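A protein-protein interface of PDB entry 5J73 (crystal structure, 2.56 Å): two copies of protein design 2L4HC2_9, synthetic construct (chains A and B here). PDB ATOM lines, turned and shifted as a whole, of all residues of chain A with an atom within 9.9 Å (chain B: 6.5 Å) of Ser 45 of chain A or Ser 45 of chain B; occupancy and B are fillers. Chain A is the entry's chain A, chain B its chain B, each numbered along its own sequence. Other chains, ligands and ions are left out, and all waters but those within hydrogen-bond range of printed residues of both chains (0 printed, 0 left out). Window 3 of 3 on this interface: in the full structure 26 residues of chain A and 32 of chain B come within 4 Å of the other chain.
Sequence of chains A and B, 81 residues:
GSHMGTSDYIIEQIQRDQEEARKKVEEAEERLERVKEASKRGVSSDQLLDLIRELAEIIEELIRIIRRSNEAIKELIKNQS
Ser 39 of chain A touches Leu 49 of chain B. Ser 45 of chain A touches Val 43 of chain B (OG to O, 3.7 Å). OG of Ser 45 of chain A touches OG of Ser 45 of chain B, 3.8 Å away. O of Ser 45 of chain A touches CD1 of Leu 48 of chain B, at 3.7 Å. Ser 45 of chain B touches Leu 48 of chain A (CA to CD1, 3.9 Å). CB of Leu 48 of chain A touches CD1 of Leu 48 of chain B, at 3.8 Å. CD2 of Leu 49 of chain A touches CD2 of Leu 48 of chain B, at 3.7 Å. Leu 48 of chain B touches Ile 52 of chain A.
Ser 45 of chain A touches just these residues of chain B: Val 43 (3.7 Å), Ser 45 (3.8 Å) and Leu 48 (3.7 Å). Of the printed residues of chain B, Ile 52 of chain A touches Leu 48. Of the printed residues of chain A, Val 43 of chain B touches Ser 45 (3.7 Å). Of chain A, only Ser 45 (3.8 Å) and Leu 48 (3.9 Å) come within 4 Å of Ser 45 of chain B. No residue of chain A comes within 4 Å of Asp 46 of chain B. Of chain A, only Ser 45, Leu 48, Leu 49 and Ile 52 come within 4 Å of Leu 48 of chain B. The nearest residue of chain B that does not touch Ser 45 of chain A is Ser 44 of chain B (5.2 Å). The nearest residue of chain A that does not touch Ser 45 of chain B is Val 43 of chain A (4.5 Å). The nearest printed residue of chain A that does not touch Val 43 of chain B is Leu 49 of chain A (5.4 Å).
Hydrophobic or aromatic side chains of chain A that line the printed part of chain B: Leu 48, Leu 49 and Ile 52. Along chain A the printed residues that touch a printed residue of chain B span positions 39 to 52. Among the printed residues, 8 pairs touch across the chains.
Ser 45 of chain A touches Val 43 of chain B, but with the chains exchanged Val 43 of chain A does not touch Ser 45 of chain B (4.5 Å). Ser 45 of chain B touches its own counterpart, Ser 45 of chain A. Leu 48 of chain B touches its own counterpart, Leu 48 of chain A. Leu 49 of chain A touches Leu 48 of chain B, but with the chains exchanged Leu 48 of chain A does not touch Leu 49 of chain B (4.4 Å). Positions printed for both chains: 43, 44, 45, 46, 47, 48, 49 and 50. Of the 8 pairs that touch across the chains among the printed residues, 4 have their exchanged pair printed and touching as well.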
ATOM      1  N   SER A  39     -29.023 -12.483  16.632  1.00  0.00           N
ATOM      2  CA  SER A  39     -29.161 -11.033  16.693  1.00  0.00           C
ATOM      3  C   SER A  39     -30.283 -10.621  17.645  1.00  0.00           C
ATOM      4  O   SER A  39     -30.142  -9.670  18.411  1.00  0.00           O
ATOM      5  CB  SER A  39     -29.421 -10.471  15.295  1.00  0.00           C
ATOM      6  OG  SER A  39     -29.872  -9.132  15.359  1.00  0.00           O
ATOM      7  N   LYS A  40     -31.398 -11.347  17.588  1.00  0.00           N
ATOM      8  CA  LYS A  40     -32.569 -11.055  18.415  1.00  0.00           C
ATOM      9  C   LYS A  40     -32.554 -11.846  19.725  1.00  0.00           C
ATOM     10  O   LYS A  40     -33.601 -12.265  20.221  1.00  0.00           O
ATOM     11  CB  LYS A  40     -33.862 -11.328  17.638  1.00  0.00           C
ATOM     12  CG  LYS A  40     -34.148 -10.314  16.537  1.00  0.00           C
ATOM     13  CD  LYS A  40     -34.411  -8.935  17.144  1.00  0.00           C
ATOM     14  CE  LYS A  40     -35.094  -7.985  16.173  1.00  0.00           C
ATOM     15  NZ  LYS A  40     -34.140  -7.375  15.212  1.00  0.00           N
ATOM     16  N   ARG A  41     -31.363 -12.046  20.275  1.00  0.00           N
ATOM     17  CA  ARG A  41     -31.191 -12.757  21.539  1.00  0.00           C
ATOM     18  C   ARG A  41     -30.606 -11.807  22.594  1.00  0.00           C
ATOM     19  O   ARG A  41     -30.189 -12.229  23.671  1.00  0.00           O
ATOM     20  CB  ARG A  41     -30.292 -13.983  21.322  1.00  0.00           C
ATOM     21  CG  ARG A  41     -30.001 -14.832  22.555  1.00  0.00           C
ATOM     22  CD  ARG A  41     -29.198 -16.068  22.197  1.00  0.00           C
ATOM     23  NE  ARG A  41     -27.847 -15.721  21.762  1.00  0.00           N
ATOM     24  CZ  ARG A  41     -26.805 -15.572  22.577  1.00  0.00           C
ATOM     25  NH1 ARG A  41     -26.948 -15.712  23.890  1.00  0.00           N
ATOM     26  NH2 ARG A  41     -25.619 -15.256  22.077  1.00  0.00           N
ATOM     27  N   GLY A  42     -30.633 -10.510  22.296  1.00  0.00           N
ATOM     28  CA  GLY A  42     -30.205  -9.498  23.249  1.00  0.00           C
ATOM     29  C   GLY A  42     -28.775  -9.731  23.695  1.00  0.00           C
ATOM     30  O   GLY A  42     -28.518 -10.198  24.805  1.00  0.00           O
ATOM     31  N   VAL A  43     -27.847  -9.384  22.814  1.00  0.00           N
ATOM     32  CA  VAL A  43     -26.424  -9.624  23.011  1.00  0.00           C
ATOM     33  C   VAL A  43     -25.681  -8.301  22.884  1.00  0.00           C
ATOM     34  O   VAL A  43     -26.265  -7.298  22.481  1.00  0.00           O
ATOM     35  CB  VAL A  43     -25.886 -10.648  22.003  1.00  0.00           C
ATOM     36  CG1 VAL A  43     -26.638 -11.954  22.155  1.00  0.00           C
ATOM     37  CG2 VAL A  43     -26.019 -10.119  20.583  1.00  0.00           C
ATOM     38  N   SER A  44     -24.392  -8.293  23.207  1.00  0.00           N
ATOM     39  CA  SER A  44     -23.687  -7.035  23.401  1.00  0.00           C
ATOM     40  C   SER A  44     -23.110  -6.516  22.092  1.00  0.00           C
ATOM     41  O   SER A  44     -23.081  -7.228  21.087  1.00  0.00           O
ATOM     42  CB  SER A  44     -22.565  -7.215  24.421  1.00  0.00           C
ATOM     43  OG  SER A  44     -21.595  -8.135  23.952  1.00  0.00           O
ATOM     44  N   SER A  45     -22.665  -5.264  22.112  1.00  0.00           N
ATOM     45  CA  SER A  45     -22.137  -4.604  20.919  1.00  0.00           C
ATOM     46  C   SER A  45     -20.987  -5.358  20.252  1.00  0.00           C
ATOM     47  O   SER A  45     -21.037  -5.612  19.051  1.00  0.00           O
ATOM     48  CB  SER A  45     -21.672  -3.188  21.271  1.00  0.00           C
ATOM     49  OG  SER A  45     -22.770  -2.357  21.607  1.00  0.00           O
ATOM     50  N   ASP A  46     -19.965  -5.713  21.027  1.00  0.00           N
ATOM     51  CA  ASP A  46     -18.823  -6.470  20.508  1.00  0.00           C
ATOM     52  C   ASP A  46     -19.275  -7.740  19.801  1.00  0.00           C
ATOM     53  O   ASP A  46     -18.683  -8.164  18.809  1.00  0.00           O
ATOM     54  CB  ASP A  46     -17.854  -6.831  21.636  1.00  0.00           C
ATOM     55  CG  ASP A  46     -17.070  -5.636  22.143  1.00  0.00           C
ATOM     56  OD1 ASP A  46     -17.093  -4.573  21.487  1.00  0.00           O
ATOM     57  OD2 ASP A  46     -16.424  -5.760  23.204  1.00  0.00           O
ATOM     58  N   GLN A  47     -20.341  -8.331  20.321  1.00  0.00           N
ATOM     59  CA  GLN A  47     -20.926  -9.533  19.745  1.00  0.00           C
ATOM     60  C   GLN A  47     -21.787  -9.214  18.532  1.00  0.00           C
ATOM     61  O   GLN A  47     -21.827  -9.989  17.579  1.00  0.00           O
ATOM     62  CB  GLN A  47     -21.741 -10.254  20.812  1.00  0.00           C
ATOM     63  CG  GLN A  47     -20.883 -10.958  21.832  1.00  0.00           C
ATOM     64  CD  GLN A  47     -21.706 -11.769  22.810  1.00  0.00           C
ATOM     65  OE1 GLN A  47     -22.534 -11.220  23.533  1.00  0.00           O
ATOM     66  NE2 GLN A  47     -21.521 -13.084  22.800  1.00  0.00           N
ATOM     67  N   LEU A  48     -22.483  -8.085  18.564  1.00  0.00           N
ATOM     68  CA  LEU A  48     -23.235  -7.643  17.398  1.00  0.00           C
ATOM     69  C   LEU A  48     -22.263  -7.297  16.275  1.00  0.00           C
ATOM     70  O   LEU A  48     -22.508  -7.608  15.110  1.00  0.00           O
ATOM     71  CB  LEU A  48     -24.113  -6.436  17.732  1.00  0.00           C
ATOM     72  CG  LEU A  48     -25.335  -6.668  18.623  1.00  0.00           C
ATOM     73  CD1 LEU A  48     -26.066  -5.355  18.833  1.00  0.00           C
ATOM     74  CD2 LEU A  48     -26.276  -7.709  18.026  1.00  0.00           C
ATOM     75  N   LEU A  49     -21.157  -6.657  16.642  1.00  0.00           N
ATOM     76  CA  LEU A  49     -20.107  -6.302  15.691  1.00  0.00           C
ATOM     77  C   LEU A  49     -19.505  -7.539  15.038  1.00  0.00           C
ATOM     78  O   LEU A  49     -19.146  -7.519  13.862  1.00  0.00           O
ATOM     79  CB  LEU A  49     -19.000  -5.500  16.385  1.00  0.00           C
ATOM     80  CG  LEU A  49     -19.322  -4.079  16.847  1.00  0.00           C
ATOM     81  CD1 LEU A  49     -18.234  -3.570  17.777  1.00  0.00           C
ATOM     82  CD2 LEU A  49     -19.458  -3.153  15.654  1.00  0.00           C
ATOM     83  N   ASP A  50     -19.391  -8.611  15.813  1.00  0.00           N
ATOM     84  CA  ASP A  50     -18.830  -9.858  15.317  1.00  0.00           C
ATOM     85  C   ASP A  50     -19.715 -10.454  14.230  1.00  0.00           C
ATOM     86  O   ASP A  50     -19.223 -10.987  13.235  1.00  0.00           O
ATOM     87  CB  ASP A  50     -18.657 -10.852  16.466  1.00  0.00           C
ATOM     88  CG  ASP A  50     -17.747 -12.006  16.108  1.00  0.00           C
ATOM     89  OD1 ASP A  50     -18.231 -12.983  15.497  1.00  0.00           O
ATOM     90  OD2 ASP A  50     -16.543 -11.937  16.436  1.00  0.00           O
ATOM     91  N   LEU A  51     -21.026 -10.361  14.425  1.00  0.00           N
ATOM     92  CA  LEU A  51     -21.982 -10.858  13.445  1.00  0.00           C
ATOM     93  C   LEU A  51     -21.926 -10.041  12.156  1.00  0.00           C
ATOM     94  O   LEU A  51     -22.056 -10.587  11.060  1.00  0.00           O
ATOM     95  CB  LEU A  51     -23.400 -10.835  14.023  1.00  0.00           C
ATOM     96  CG  LEU A  51     -23.655 -11.702  15.263  1.00  0.00           C
ATOM     97  CD1 LEU A  51     -25.129 -11.666  15.636  1.00  0.00           C
ATOM     98  CD2 LEU A  51     -23.190 -13.138  15.063  1.00  0.00           C
ATOM     99  N   ILE A  52     -21.740  -8.732  12.296  1.00  0.00           N
ATOM    100  CA  ILE A  52     -21.622  -7.834  11.150  1.00  0.00           C
ATOM    101  C   ILE A  52     -20.389  -8.178  10.313  1.00  0.00           C
ATOM    102  O   ILE A  52     -20.451  -8.193   9.083  1.00  0.00           O
ATOM    103  CB  ILE A  52     -21.570  -6.360  11.611  1.00  0.00           C
ATOM    104  CG1 ILE A  52     -22.942  -5.948  12.155  1.00  0.00           C
ATOM    105  CG2 ILE A  52     -21.122  -5.445  10.470  1.00  0.00           C
ATOM    106  CD1 ILE A  52     -23.030  -4.518  12.661  1.00  0.00           C
ATOM    107  N   ARG A  53     -19.273  -8.446  10.983  1.00  0.00           N
ATOM    108  CA  ARG A  53     -18.052  -8.885  10.314  1.00  0.00           C
ATOM    109  C   ARG A  53     -18.297 -10.203   9.581  1.00  0.00           C
ATOM    110  O   ARG A  53     -17.833 -10.404   8.458  1.00  0.00           O
ATOM    111  CB  ARG A  53     -16.915  -9.024  11.334  1.00  0.00           C
ATOM    112  CG  ARG A  53     -16.312  -7.684  11.738  1.00  0.00           C
ATOM    113  CD  ARG A  53     -15.113  -7.796  12.684  1.00  0.00           C
ATOM    114  NE  ARG A  53     -13.996  -8.580  12.159  1.00  0.00           N
ATOM    115  CZ  ARG A  53     -13.650  -9.792  12.591  1.00  0.00           C
ATOM    116  NH1 ARG A  53     -14.317 -10.385  13.576  1.00  0.00           N
ATOM    117  NH2 ARG A  53     -12.611 -10.412  12.046  1.00  0.00           N
ATOM    118  N   VAL B  43     -20.988   2.619  19.222  1.00  0.00           N
ATOM    119  CA  VAL B  43     -22.347   2.938  18.790  1.00  0.00           C
ATOM    120  C   VAL B  43     -23.379   2.051  19.464  1.00  0.00           C
ATOM    121  O   VAL B  43     -23.058   1.007  20.036  1.00  0.00           O
ATOM    122  CB  VAL B  43     -22.517   2.794  17.254  1.00  0.00           C
ATOM    123  CG1 VAL B  43     -21.616   3.769  16.522  1.00  0.00           C
ATOM    124  CG2 VAL B  43     -22.267   1.345  16.799  1.00  0.00           C
ATOM    125  N   SER B  44     -24.633   2.463  19.339  1.00  0.00           N
ATOM    126  CA  SER B  44     -25.718   1.931  20.145  1.00  0.00           C
ATOM    127  C   SER B  44     -26.403   0.753  19.482  1.00  0.00           C
ATOM    128  O   SER B  44     -26.913   0.876  18.371  1.00  0.00           O
ATOM    129  CB  SER B  44     -26.751   3.029  20.400  1.00  0.00           C
ATOM    130  OG  SER B  44     -27.318   3.465  19.174  1.00  0.00           O
ATOM    131  N   SER B  45     -26.347  -0.396  20.159  1.00  0.00           N
ATOM    132  CA  SER B  45     -26.989  -1.646  19.737  1.00  0.00           C
ATOM    133  C   SER B  45     -28.091  -1.470  18.694  1.00  0.00           C
ATOM    134  O   SER B  45     -28.074  -2.128  17.654  1.00  0.00           O
ATOM    135  CB  SER B  45     -27.581  -2.355  20.962  1.00  0.00           C
ATOM    136  OG  SER B  45     -26.560  -2.832  21.824  1.00  0.00           O
ATOM    137  N   ASP B  46     -29.025  -0.572  18.972  1.00  0.00           N
ATOM    138  CA  ASP B  46     -30.122  -0.266  18.059  1.00  0.00           C
ATOM    139  C   ASP B  46     -29.664   0.076  16.650  1.00  0.00           C
ATOM    140  O   ASP B  46     -30.315  -0.279  15.675  1.00  0.00           O
ATOM    141  CB  ASP B  46     -30.970   0.873  18.608  1.00  0.00           C
ATOM    142  CG  ASP B  46     -31.809   0.468  19.796  1.00  0.00           C
ATOM    143  OD1 ASP B  46     -31.934  -0.748  20.064  1.00  0.00           O
ATOM    144  OD2 ASP B  46     -32.347   1.367  20.474  1.00  0.00           O
ATOM    145  N   GLN B  47     -28.534   0.778  16.539  1.00  0.00           N
ATOM    146  CA  GLN B  47     -27.994   1.107  15.227  1.00  0.00           C
ATOM    147  C   GLN B  47     -27.225  -0.089  14.673  1.00  0.00           C
ATOM    148  O   GLN B  47     -27.217  -0.310  13.463  1.00  0.00           O
ATOM    149  CB  GLN B  47     -27.102   2.351  15.295  1.00  0.00           C
ATOM    150  CG  GLN B  47     -27.907   3.620  15.548  1.00  0.00           C
ATOM    151  CD  GLN B  47     -27.102   4.893  15.376  1.00  0.00           C
ATOM    152  OE1 GLN B  47     -25.880   4.898  15.527  1.00  0.00           O
ATOM    153  NE2 GLN B  47     -27.789   5.984  15.046  1.00  0.00           N
ATOM    154  N   LEU B  48     -26.580  -0.856  15.542  1.00  0.00           N
ATOM    155  CA  LEU B  48     -25.918  -2.077  15.096  1.00  0.00           C
ATOM    156  C   LEU B  48     -26.982  -3.043  14.585  1.00  0.00           C
ATOM    157  O   LEU B  48     -26.758  -3.764  13.613  1.00  0.00           O
ATOM    158  CB  LEU B  48     -25.094  -2.724  16.210  1.00  0.00           C
ATOM    159  CG  LEU B  48     -23.819  -2.000  16.653  1.00  0.00           C
ATOM    160  CD1 LEU B  48     -23.113  -2.804  17.732  1.00  0.00           C
ATOM    161  CD2 LEU B  48     -22.878  -1.724  15.485  1.00  0.00           C
ATOM    162  N   LEU B  49     -28.134  -3.064  15.252  1.00  0.00           N
ATOM    163  CA  LEU B  49     -29.250  -3.899  14.819  1.00  0.00           C
ATOM    164  C   LEU B  49     -29.705  -3.491  13.418  1.00  0.00           C
ATOM    165  O   LEU B  49     -30.102  -4.336  12.615  1.00  0.00           O
ATOM    166  CB  LEU B  49     -30.430  -3.805  15.795  1.00  0.00           C
ATOM    167  CG  LEU B  49     -30.273  -4.396  17.200  1.00  0.00           C
ATOM    168  CD1 LEU B  49     -31.438  -3.969  18.092  1.00  0.00           C
ATOM    169  CD2 LEU B  49     -30.160  -5.912  17.164  1.00  0.00           C
ATOM    170  N   ASP B  50     -29.661  -2.190  13.137  1.00  0.00           N
ATOM    171  CA  ASP B  50     -30.053  -1.674  11.827  1.00  0.00           C
ATOM    172  C   ASP B  50     -29.100  -2.133  10.727  1.00  0.00           C
ATOM    173  O   ASP B  50     -29.530  -2.466   9.622  1.00  0.00           O
ATOM    174  CB  ASP B  50     -30.106  -0.142  11.841  1.00  0.00           C
ATOM    175  CG  ASP B  50     -31.245   0.403  12.682  1.00  0.00           C
ATOM    176  OD1 ASP B  50     -32.257  -0.304  12.861  1.00  0.00           O
ATOM    177  OD2 ASP B  50     -31.134   1.555  13.148  1.00  0.00           O
